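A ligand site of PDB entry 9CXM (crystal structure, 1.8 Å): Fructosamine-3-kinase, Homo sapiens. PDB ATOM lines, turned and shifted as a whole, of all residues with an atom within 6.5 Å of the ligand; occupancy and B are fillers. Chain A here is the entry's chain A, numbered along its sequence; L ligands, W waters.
N of Leu 92 lies within hydrogen-bond range of N4 of the ligand (2.9 Å). The side-chain carboxylate of Asp 216 lies close to an oxygen (O1) of the ligand (3.1 Å). O5 of the ligand lies close to OD1 of Asn 204 (3.2 Å). The backbone carbonyl oxygen (O) of Glu 90 sits at hydrogen-bond distance from a nitrogen (N3) of the ligand, at 2.9 Å. NZ of Lys 42 is in salt-bridge range of O4 of the ligand, 2.6 Å away. The side-chain sulfur (SD) of Met 89 sits close to a nitrogen (N3) of the ligand (3.6 Å). N of Ser 27 is in hydrogen-bond range of O3 of the ligand (2.8 Å). O9 of the ligand lies within hydrogen-bond range of OH of Tyr 215, 3.3 Å away. The side-chain hydroxyl of Ser 27 is in hydrogen-bond range of an oxygen (O3) of the ligand, at 3.4 Å.
Water W2 lies within hydrogen-bond range of an oxygen (O5) of the ligand (2.6 Å), the backbone carbonyl oxygen of Gly 203 (2.8 Å) and the side-chain amide oxygen of Asn 204 (3.3 Å). Water W4 lies within hydrogen-bond range of an oxygen (O4) of the ligand (2.8 Å), the side-chain sulfur (SD) of Met 89 (3.5 Å) and the side-chain amino group (NZ) of Lys 42 (3.5 Å). Water W1 lies within hydrogen-bond range of OD2 of Asp 216, OD1 of Asn 204 and O5 of the ligand.
Phe 40 touches the ligand. CB of Pro 72 touches N3 of the ligand (3.5 Å). His 91 touches the ligand (CD2 to C9, 3.4 Å). Met 94 touches the ligand (CE to C4, 3.5 Å). Of the 22 residues printed, 12 come within 4 Å of the ligand. The nearest printed residue that does not touch the ligand is Gly 203 (4.04 Å).
The backbone carbonyl oxygen (O) of Arg 73 lies within hydrogen-bond range of the backbone NH (N) of Glu 90. OD2 of Asp 216 sits close to OD1 of Asn 204 (3.3 Å). The backbone carbonyl oxygen (O) of Gly 203 is in hydrogen-bond range of the side-chain hydroxyl (OH) of Tyr 215, at 2.8 Å. NZ of Lys 42 lies within salt-bridge range of OD1 of Asp 216 (3.4 Å). The side-chain amino group (NZ) of Lys 42 lies within salt-bridge range of the side-chain carboxylate (OE2) of Glu 56 (2.6 Å). O of Asn 204 sits at hydrogen-bond distance from N of Tyr 215 (3.0 Å). The backbone NH (N) of Met 89 lies within hydrogen-bond range of the backbone carbonyl oxygen (O) of Phe 40.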
ATOM      1  N   SER A  27      -9.314  -1.077  33.733  1.00  0.00           N
ATOM      2  CA  SER A  27      -8.501   0.089  34.061  1.00  0.00           C
ATOM      3  C   SER A  27      -9.342   1.172  34.731  1.00  0.00           C
ATOM      4  O   SER A  27      -9.904   2.030  34.043  1.00  0.00           O
ATOM      5  CB  SER A  27      -7.830   0.654  32.812  1.00  0.00           C
ATOM      6  OG  SER A  27      -7.081  -0.333  32.117  1.00  0.00           O
ATOM      7  N   GLU A  28      -9.409   1.128  36.081  1.00  0.00           N
ATOM      8  CA  GLU A  28     -10.096   2.146  36.900  1.00  0.00           C
ATOM      9  C   GLU A  28     -11.517   2.400  36.399  1.00  0.00           C
ATOM     10  O   GLU A  28     -11.976   3.544  36.320  1.00  0.00           O
ATOM     11  CB  GLU A  28      -9.291   3.441  36.961  1.00  0.00           C
ATOM     12  N   GLY A  29     -12.251   1.336  36.106  1.00  0.00           N
ATOM     13  CA  GLY A  29     -13.567   1.459  35.536  1.00  0.00           C
ATOM     14  C   GLY A  29     -14.576   1.368  36.660  1.00  0.00           C
ATOM     15  O   GLY A  29     -14.557   0.421  37.451  1.00  0.00           O
ATOM     16  N   ALA A  31     -18.764   1.996  37.758  1.00  0.00           N
ATOM     17  CA  ALA A  31     -20.148   2.216  37.327  1.00  0.00           C
ATOM     18  C   ALA A  31     -20.728   3.272  38.257  1.00  0.00           C
ATOM     19  O   ALA A  31     -20.286   3.336  39.417  1.00  0.00           O
ATOM     20  CB  ALA A  31     -20.926   0.938  37.416  1.00  0.00           C
ATOM     21  N   VAL A  39     -24.820   4.395  33.953  1.00  0.00           N
ATOM     22  CA  VAL A  39     -23.681   4.564  33.053  1.00  0.00           C
ATOM     23  C   VAL A  39     -22.495   3.823  33.629  1.00  0.00           C
ATOM     24  O   VAL A  39     -22.412   3.537  34.832  1.00  0.00           O
ATOM     25  CB  VAL A  39     -23.299   6.046  32.796  1.00  0.00           C
ATOM     26  CG1 VAL A  39     -24.426   6.829  32.223  1.00  0.00           C
ATOM     27  CG2 VAL A  39     -22.667   6.683  34.060  1.00  0.00           C
ATOM     28  N   PHE A  40     -21.556   3.509  32.738  1.00  0.00           N
ATOM     29  CA  PHE A  40     -20.281   2.943  33.102  1.00  0.00           C
ATOM     30  C   PHE A  40     -19.198   3.863  32.572  1.00  0.00           C
ATOM     31  O   PHE A  40     -19.260   4.307  31.420  1.00  0.00           O
ATOM     32  CB  PHE A  40     -20.122   1.505  32.547  1.00  0.00           C
ATOM     33  CG  PHE A  40     -18.914   0.819  33.009  1.00  0.00           C
ATOM     34  CD1 PHE A  40     -18.872   0.202  34.253  1.00  0.00           C
ATOM     35  CD2 PHE A  40     -17.771   0.801  32.231  1.00  0.00           C
ATOM     36  CE1 PHE A  40     -17.712  -0.429  34.690  1.00  0.00           C
ATOM     37  CE2 PHE A  40     -16.638   0.166  32.652  1.00  0.00           C
ATOM     38  CZ  PHE A  40     -16.582  -0.445  33.876  1.00  0.00           C
ATOM     39  N   LYS A  42     -15.073   4.564  32.090  1.00  0.00           N
ATOM     40  CA  LYS A  42     -13.694   4.095  32.063  1.00  0.00           C
ATOM     41  C   LYS A  42     -12.767   5.296  32.199  1.00  0.00           C
ATOM     42  O   LYS A  42     -12.974   6.325  31.575  1.00  0.00           O
ATOM     43  CB  LYS A  42     -13.305   3.339  30.768  1.00  0.00           C
ATOM     44  CG  LYS A  42     -13.919   1.950  30.618  1.00  0.00           C
ATOM     45  CD  LYS A  42     -13.887   1.518  29.093  1.00  0.00           C
ATOM     46  CE  LYS A  42     -13.063   0.315  28.893  1.00  0.00           C
ATOM     47  NZ  LYS A  42     -13.137  -0.230  27.498  1.00  0.00           N
ATOM     48  N   VAL A  43     -11.742   5.150  33.012  1.00  0.00           N
ATOM     49  CA  VAL A  43     -10.845   6.255  33.301  1.00  0.00           C
ATOM     50  C   VAL A  43      -9.444   5.817  32.944  1.00  0.00           C
ATOM     51  O   VAL A  43      -9.032   4.703  33.268  1.00  0.00           O
ATOM     52  CB  VAL A  43     -10.938   6.676  34.783  1.00  0.00           C
ATOM     53  CG1 VAL A  43      -9.776   7.551  35.098  1.00  0.00           C
ATOM     54  CG2 VAL A  43     -12.295   7.325  35.077  1.00  0.00           C
ATOM     55  N   GLU A  56     -11.829   3.522  20.398  1.00  0.00           N
ATOM     56  CA  GLU A  56     -12.832   2.603  20.936  1.00  0.00           C
ATOM     57  C   GLU A  56     -14.205   3.077  20.529  1.00  0.00           C
ATOM     58  O   GLU A  56     -15.061   2.253  20.169  1.00  0.00           O
ATOM     59  CB  GLU A  56     -12.741   2.511  22.463  1.00  0.00           C
ATOM     60  CG  GLU A  56     -13.632   1.429  23.048  1.00  0.00           C
ATOM     61  CD  GLU A  56     -13.408   1.240  24.557  1.00  0.00           C
ATOM     62  OE1 GLU A  56     -12.443   1.866  25.078  1.00  0.00           O
ATOM     63  OE2 GLU A  56     -14.198   0.492  25.199  1.00  0.00           O
ATOM     64  N   PRO A  72     -21.975  -1.782  24.071  1.00  0.00           N
ATOM     65  CA  PRO A  72     -22.429  -0.624  24.869  1.00  0.00           C
ATOM     66  C   PRO A  72     -22.429   0.634  24.004  1.00  0.00           C
ATOM     67  O   PRO A  72     -21.544   0.839  23.172  1.00  0.00           O
ATOM     68  CB  PRO A  72     -21.397  -0.554  26.010  1.00  0.00           C
ATOM     69  CG  PRO A  72     -20.281  -1.384  25.650  1.00  0.00           C
ATOM     70  CD  PRO A  72     -20.777  -2.417  24.614  1.00  0.00           C
ATOM     71  N   ARG A  73     -23.451   1.468  24.174  1.00  0.00           N
ATOM     72  CA  ARG A  73     -23.550   2.704  23.387  1.00  0.00           C
ATOM     73  C   ARG A  73     -22.586   3.731  23.945  1.00  0.00           C
ATOM     74  O   ARG A  73     -22.689   4.097  25.120  1.00  0.00           O
ATOM     75  CB  ARG A  73     -24.979   3.259  23.433  1.00  0.00           C
ATOM     76  CG  ARG A  73     -25.141   4.454  22.482  1.00  0.00           C
ATOM     77  CD  ARG A  73     -26.559   5.037  22.471  1.00  0.00           C
ATOM     78  NE  ARG A  73     -26.931   5.495  23.812  1.00  0.00           N
ATOM     79  CZ  ARG A  73     -26.815   6.738  24.249  1.00  0.00           C
ATOM     80  NH1 ARG A  73     -26.298   7.703  23.487  1.00  0.00           N
ATOM     81  NH2 ARG A  73     -27.196   7.038  25.491  1.00  0.00           N
ATOM     82  N   MET A  89     -20.133   5.391  28.917  1.00  0.00           N
ATOM     83  CA  MET A  89     -20.960   4.607  28.014  1.00  0.00           C
ATOM     84  C   MET A  89     -22.205   4.087  28.743  1.00  0.00           C
ATOM     85  O   MET A  89     -22.268   4.086  29.977  1.00  0.00           O
ATOM     86  CB  MET A  89     -20.133   3.441  27.425  1.00  0.00           C
ATOM     87  CG  MET A  89     -19.759   2.319  28.377  1.00  0.00           C
ATOM     88  SD  MET A  89     -18.573   1.247  27.544  1.00  0.00           S
ATOM     89  CE  MET A  89     -17.032   1.988  27.984  1.00  0.00           C
ATOM     90  N   GLU A  90     -23.181   3.630  27.955  1.00  0.00           N
ATOM     91  CA  GLU A  90     -24.360   2.947  28.487  1.00  0.00           C
ATOM     92  C   GLU A  90     -23.936   1.806  29.403  1.00  0.00           C
ATOM     93  O   GLU A  90     -23.031   1.039  29.093  1.00  0.00           O
ATOM     94  CB  GLU A  90     -25.165   2.379  27.291  1.00  0.00           C
ATOM     95  CG  GLU A  90     -26.326   1.460  27.664  1.00  0.00           C
ATOM     96  CD  GLU A  90     -26.790   0.685  26.465  1.00  0.00           C
ATOM     97  OE1 GLU A  90     -25.958   0.462  25.525  1.00  0.00           O
ATOM     98  OE2 GLU A  90     -27.978   0.357  26.398  1.00  0.00           O
ATOM     99  N   HIS A  91     -24.574   1.704  30.566  1.00  0.00           N
ATOM    100  CA  HIS A  91     -24.281   0.599  31.463  1.00  0.00           C
ATOM    101  C   HIS A  91     -25.107  -0.614  31.069  1.00  0.00           C
ATOM    102  O   HIS A  91     -26.284  -0.482  30.700  1.00  0.00           O
ATOM    103  CB  HIS A  91     -24.591   0.981  32.913  1.00  0.00           C
ATOM    104  CG  HIS A  91     -24.309  -0.102  33.897  1.00  0.00           C
ATOM    105  ND1 HIS A  91     -25.238  -1.076  34.212  1.00  0.00           N
ATOM    106  CD2 HIS A  91     -23.181  -0.425  34.577  1.00  0.00           C
ATOM    107  CE1 HIS A  91     -24.710  -1.917  35.089  1.00  0.00           C
ATOM    108  NE2 HIS A  91     -23.459  -1.539  35.318  1.00  0.00           N
ATOM    109  N   LEU A  92     -24.469  -1.773  31.131  1.00  0.00           N
ATOM    110  CA  LEU A  92     -25.163  -3.041  30.804  1.00  0.00           C
ATOM    111  C   LEU A  92     -24.917  -4.048  31.930  1.00  0.00           C
ATOM    112  O   LEU A  92     -23.762  -4.237  32.319  1.00  0.00           O
ATOM    113  CB  LEU A  92     -24.634  -3.561  29.463  1.00  0.00           C
ATOM    114  CG  LEU A  92     -24.961  -2.703  28.239  1.00  0.00           C
ATOM    115  CD1 LEU A  92     -24.158  -3.168  27.035  1.00  0.00           C
ATOM    116  CD2 LEU A  92     -26.448  -2.753  27.925  1.00  0.00           C
ATOM    117  N   LYS A  93     -25.998  -4.640  32.453  1.00  0.00           N
ATOM    118  CA  LYS A  93     -25.870  -5.703  33.479  1.00  0.00           C
ATOM    119  C   LYS A  93     -25.392  -6.931  32.726  1.00  0.00           C
ATOM    120  O   LYS A  93     -26.108  -7.354  31.823  1.00  0.00           O
ATOM    121  CB  LYS A  93     -27.219  -5.921  34.182  1.00  0.00           C
ATOM    122  N   MET A  94     -24.221  -7.429  33.079  1.00  0.00           N
ATOM    123  CA  MET A  94     -23.644  -8.518  32.263  1.00  0.00           C
ATOM    124  C   MET A  94     -23.175  -9.684  33.122  1.00  0.00           C
ATOM    125  O   MET A  94     -22.849  -9.471  34.301  1.00  0.00           O
ATOM    126  CB  MET A  94     -22.436  -7.964  31.505  1.00  0.00           C
ATOM    127  CG  MET A  94     -22.759  -6.851  30.557  1.00  0.00           C
ATOM    128  SD  MET A  94     -21.252  -6.329  29.710  1.00  0.00           S
ATOM    129  CE  MET A  94     -20.166  -6.061  31.101  1.00  0.00           C
ATOM    130  N   TRP A 201     -11.121 -11.463  23.167  1.00  0.00           N
ATOM    131  CA  TRP A 201     -10.759 -12.288  24.317  1.00  0.00           C
ATOM    132  C   TRP A 201     -12.015 -12.609  25.143  1.00  0.00           C
ATOM    133  O   TRP A 201     -13.003 -11.869  25.143  1.00  0.00           O
ATOM    134  CB  TRP A 201      -9.694 -11.545  25.140  1.00  0.00           C
ATOM    135  CG  TRP A 201      -9.492 -11.949  26.571  1.00  0.00           C
ATOM    136  CD1 TRP A 201      -9.184 -13.185  27.027  1.00  0.00           C
ATOM    137  CD2 TRP A 201      -9.470 -11.088  27.705  1.00  0.00           C
ATOM    138  NE1 TRP A 201      -9.030 -13.175  28.385  1.00  0.00           N
ATOM    139  CE2 TRP A 201      -9.195 -11.889  28.829  1.00  0.00           C
ATOM    140  CE3 TRP A 201      -9.683  -9.724  27.885  1.00  0.00           C
ATOM    141  CZ2 TRP A 201      -9.128 -11.370  30.123  1.00  0.00           C
ATOM    142  CZ3 TRP A 201      -9.626  -9.196  29.175  1.00  0.00           C
ATOM    143  CH2 TRP A 201      -9.344 -10.023  30.275  1.00  0.00           C
ATOM    144  N   GLY A 203     -12.526 -12.210  28.064  1.00  0.00           N
ATOM    145  CA  GLY A 203     -12.822 -11.140  29.006  1.00  0.00           C
ATOM    146  C   GLY A 203     -13.542  -9.965  28.391  1.00  0.00           C
ATOM    147  O   GLY A 203     -13.934  -9.052  29.116  1.00  0.00           O
ATOM    148  N   ASN A 204     -13.676  -9.925  27.068  1.00  0.00           N
ATOM    149  CA  ASN A 204     -14.380  -8.825  26.401  1.00  0.00           C
ATOM    150  C   ASN A 204     -15.730  -9.252  25.854  1.00  0.00           C
ATOM    151  O   ASN A 204     -16.307  -8.550  25.000  1.00  0.00           O
ATOM    152  CB  ASN A 204     -13.498  -8.272  25.269  1.00  0.00           C
ATOM    153  CG  ASN A 204     -12.358  -7.441  25.781  1.00  0.00           C
ATOM    154  OD1 ASN A 204     -12.393  -6.964  26.945  1.00  0.00           O
ATOM    155  ND2 ASN A 204     -11.349  -7.245  24.949  1.00  0.00           N
ATOM    156  N   TYR A 215     -17.618  -6.017  23.924  1.00  0.00           N
ATOM    157  CA  TYR A 215     -17.195  -4.657  24.290  1.00  0.00           C
ATOM    158  C   TYR A 215     -15.672  -4.571  24.212  1.00  0.00           C
ATOM    159  O   TYR A 215     -14.986  -5.549  23.881  1.00  0.00           O
ATOM    160  CB  TYR A 215     -17.745  -4.271  25.713  1.00  0.00           C
ATOM    161  CG  TYR A 215     -17.426  -5.340  26.755  1.00  0.00           C
ATOM    162  CD1 TYR A 215     -16.227  -5.330  27.444  1.00  0.00           C
ATOM    163  CD2 TYR A 215     -18.366  -6.312  27.078  1.00  0.00           C
ATOM    164  CE1 TYR A 215     -15.926  -6.306  28.363  1.00  0.00           C
ATOM    165  CE2 TYR A 215     -18.078  -7.276  28.002  1.00  0.00           C
ATOM    166  CZ  TYR A 215     -16.877  -7.269  28.639  1.00  0.00           C
ATOM    167  OH  TYR A 215     -16.599  -8.234  29.561  1.00  0.00           O
ATOM    168  N   ASP A 216     -15.127  -3.367  24.488  1.00  0.00           N
ATOM    169  CA  ASP A 216     -13.697  -3.107  24.408  1.00  0.00           C
ATOM    170  C   ASP A 216     -13.117  -3.490  23.035  1.00  0.00           C
ATOM    171  O   ASP A 216     -12.074  -4.119  22.945  1.00  0.00           O
ATOM    172  CB  ASP A 216     -12.959  -3.908  25.484  1.00  0.00           C
ATOM    173  CG  ASP A 216     -11.609  -3.339  25.816  1.00  0.00           C
ATOM    174  OD1 ASP A 216     -11.295  -2.174  25.442  1.00  0.00           O
ATOM    175  OD2 ASP A 216     -10.860  -4.052  26.503  1.00  0.00           O
HETATM  176  P1  LIG L   1     -10.509  -2.273  30.070  1.00  0.00           P
HETATM  177  O1  LIG L   1     -10.344  -1.887  28.606  1.00  0.00           O
HETATM  178  O2  LIG L   1      -9.926  -3.605  30.469  1.00  0.00           O
HETATM  179  O3  LIG L   1     -10.162  -1.159  31.061  1.00  0.00           O
HETATM  180  P2  LIG L   1     -13.154  -3.364  29.557  1.00  0.00           P
HETATM  181  O4  LIG L   1     -13.893  -2.541  28.528  1.00  0.00           O
HETATM  182  O5  LIG L   1     -12.451  -4.660  29.193  1.00  0.00           O
HETATM  183  O6  LIG L   1     -12.084  -2.441  30.357  1.00  0.00           O
HETATM  184  O7  LIG L   1     -14.245  -3.621  30.723  1.00  0.00           O
HETATM  185  C1  LIG L   1     -13.753  -4.246  31.930  1.00  0.00           C
HETATM  186  C2  LIG L   1     -14.914  -4.686  32.818  1.00  0.00           C
HETATM  187  O8  LIG L   1     -15.805  -3.612  33.118  1.00  0.00           O
HETATM  188  C3  LIG L   1     -15.788  -5.704  32.131  1.00  0.00           C
HETATM  189  O9  LIG L   1     -15.237  -7.000  32.344  1.00  0.00           O
HETATM  190  C4  LIG L   1     -17.164  -5.519  32.716  1.00  0.00           C
HETATM  191  O10 LIG L   1     -17.336  -6.264  33.941  1.00  0.00           O
HETATM  192  C5  LIG L   1     -17.163  -4.042  33.057  1.00  0.00           C
HETATM  193  N1  LIG L   1     -17.825  -3.253  31.970  1.00  0.00           N
HETATM  194  C6  LIG L   1     -17.218  -2.800  30.850  1.00  0.00           C
HETATM  195  N2  LIG L   1     -18.072  -2.086  30.084  1.00  0.00           N
HETATM  196  C7  LIG L   1     -19.255  -2.091  30.732  1.00  0.00           C
HETATM  197  C8  LIG L   1     -20.592  -1.542  30.505  1.00  0.00           C
HETATM  198  N3  LIG L   1     -20.847  -0.827  29.408  1.00  0.00           N
HETATM  199  N4  LIG L   1     -21.548  -1.746  31.427  1.00  0.00           N
HETATM  200  C9  LIG L   1     -21.298  -2.456  32.543  1.00  0.00           C
HETATM  201  N5  LIG L   1     -20.118  -2.992  32.823  1.00  0.00           N
HETATM  202  C10 LIG L   1     -19.083  -2.851  31.979  1.00  0.00           C
HETATM  203  O   HOH W   1      -9.715  -5.917  28.229  1.00  0.00           O
HETATM  204  O   HOH W   2     -12.350  -6.983  30.252  1.00  0.00           O
HETATM  205  O   HOH W   3     -20.451  -4.203  35.194  1.00  0.00           O
HETATM  206  O   HOH W   4     -16.383  -1.433  27.904  1.00  0.00           O
HETATM  207  O   HOH W   5      -9.769   0.675  28.581  1.00  0.00           O
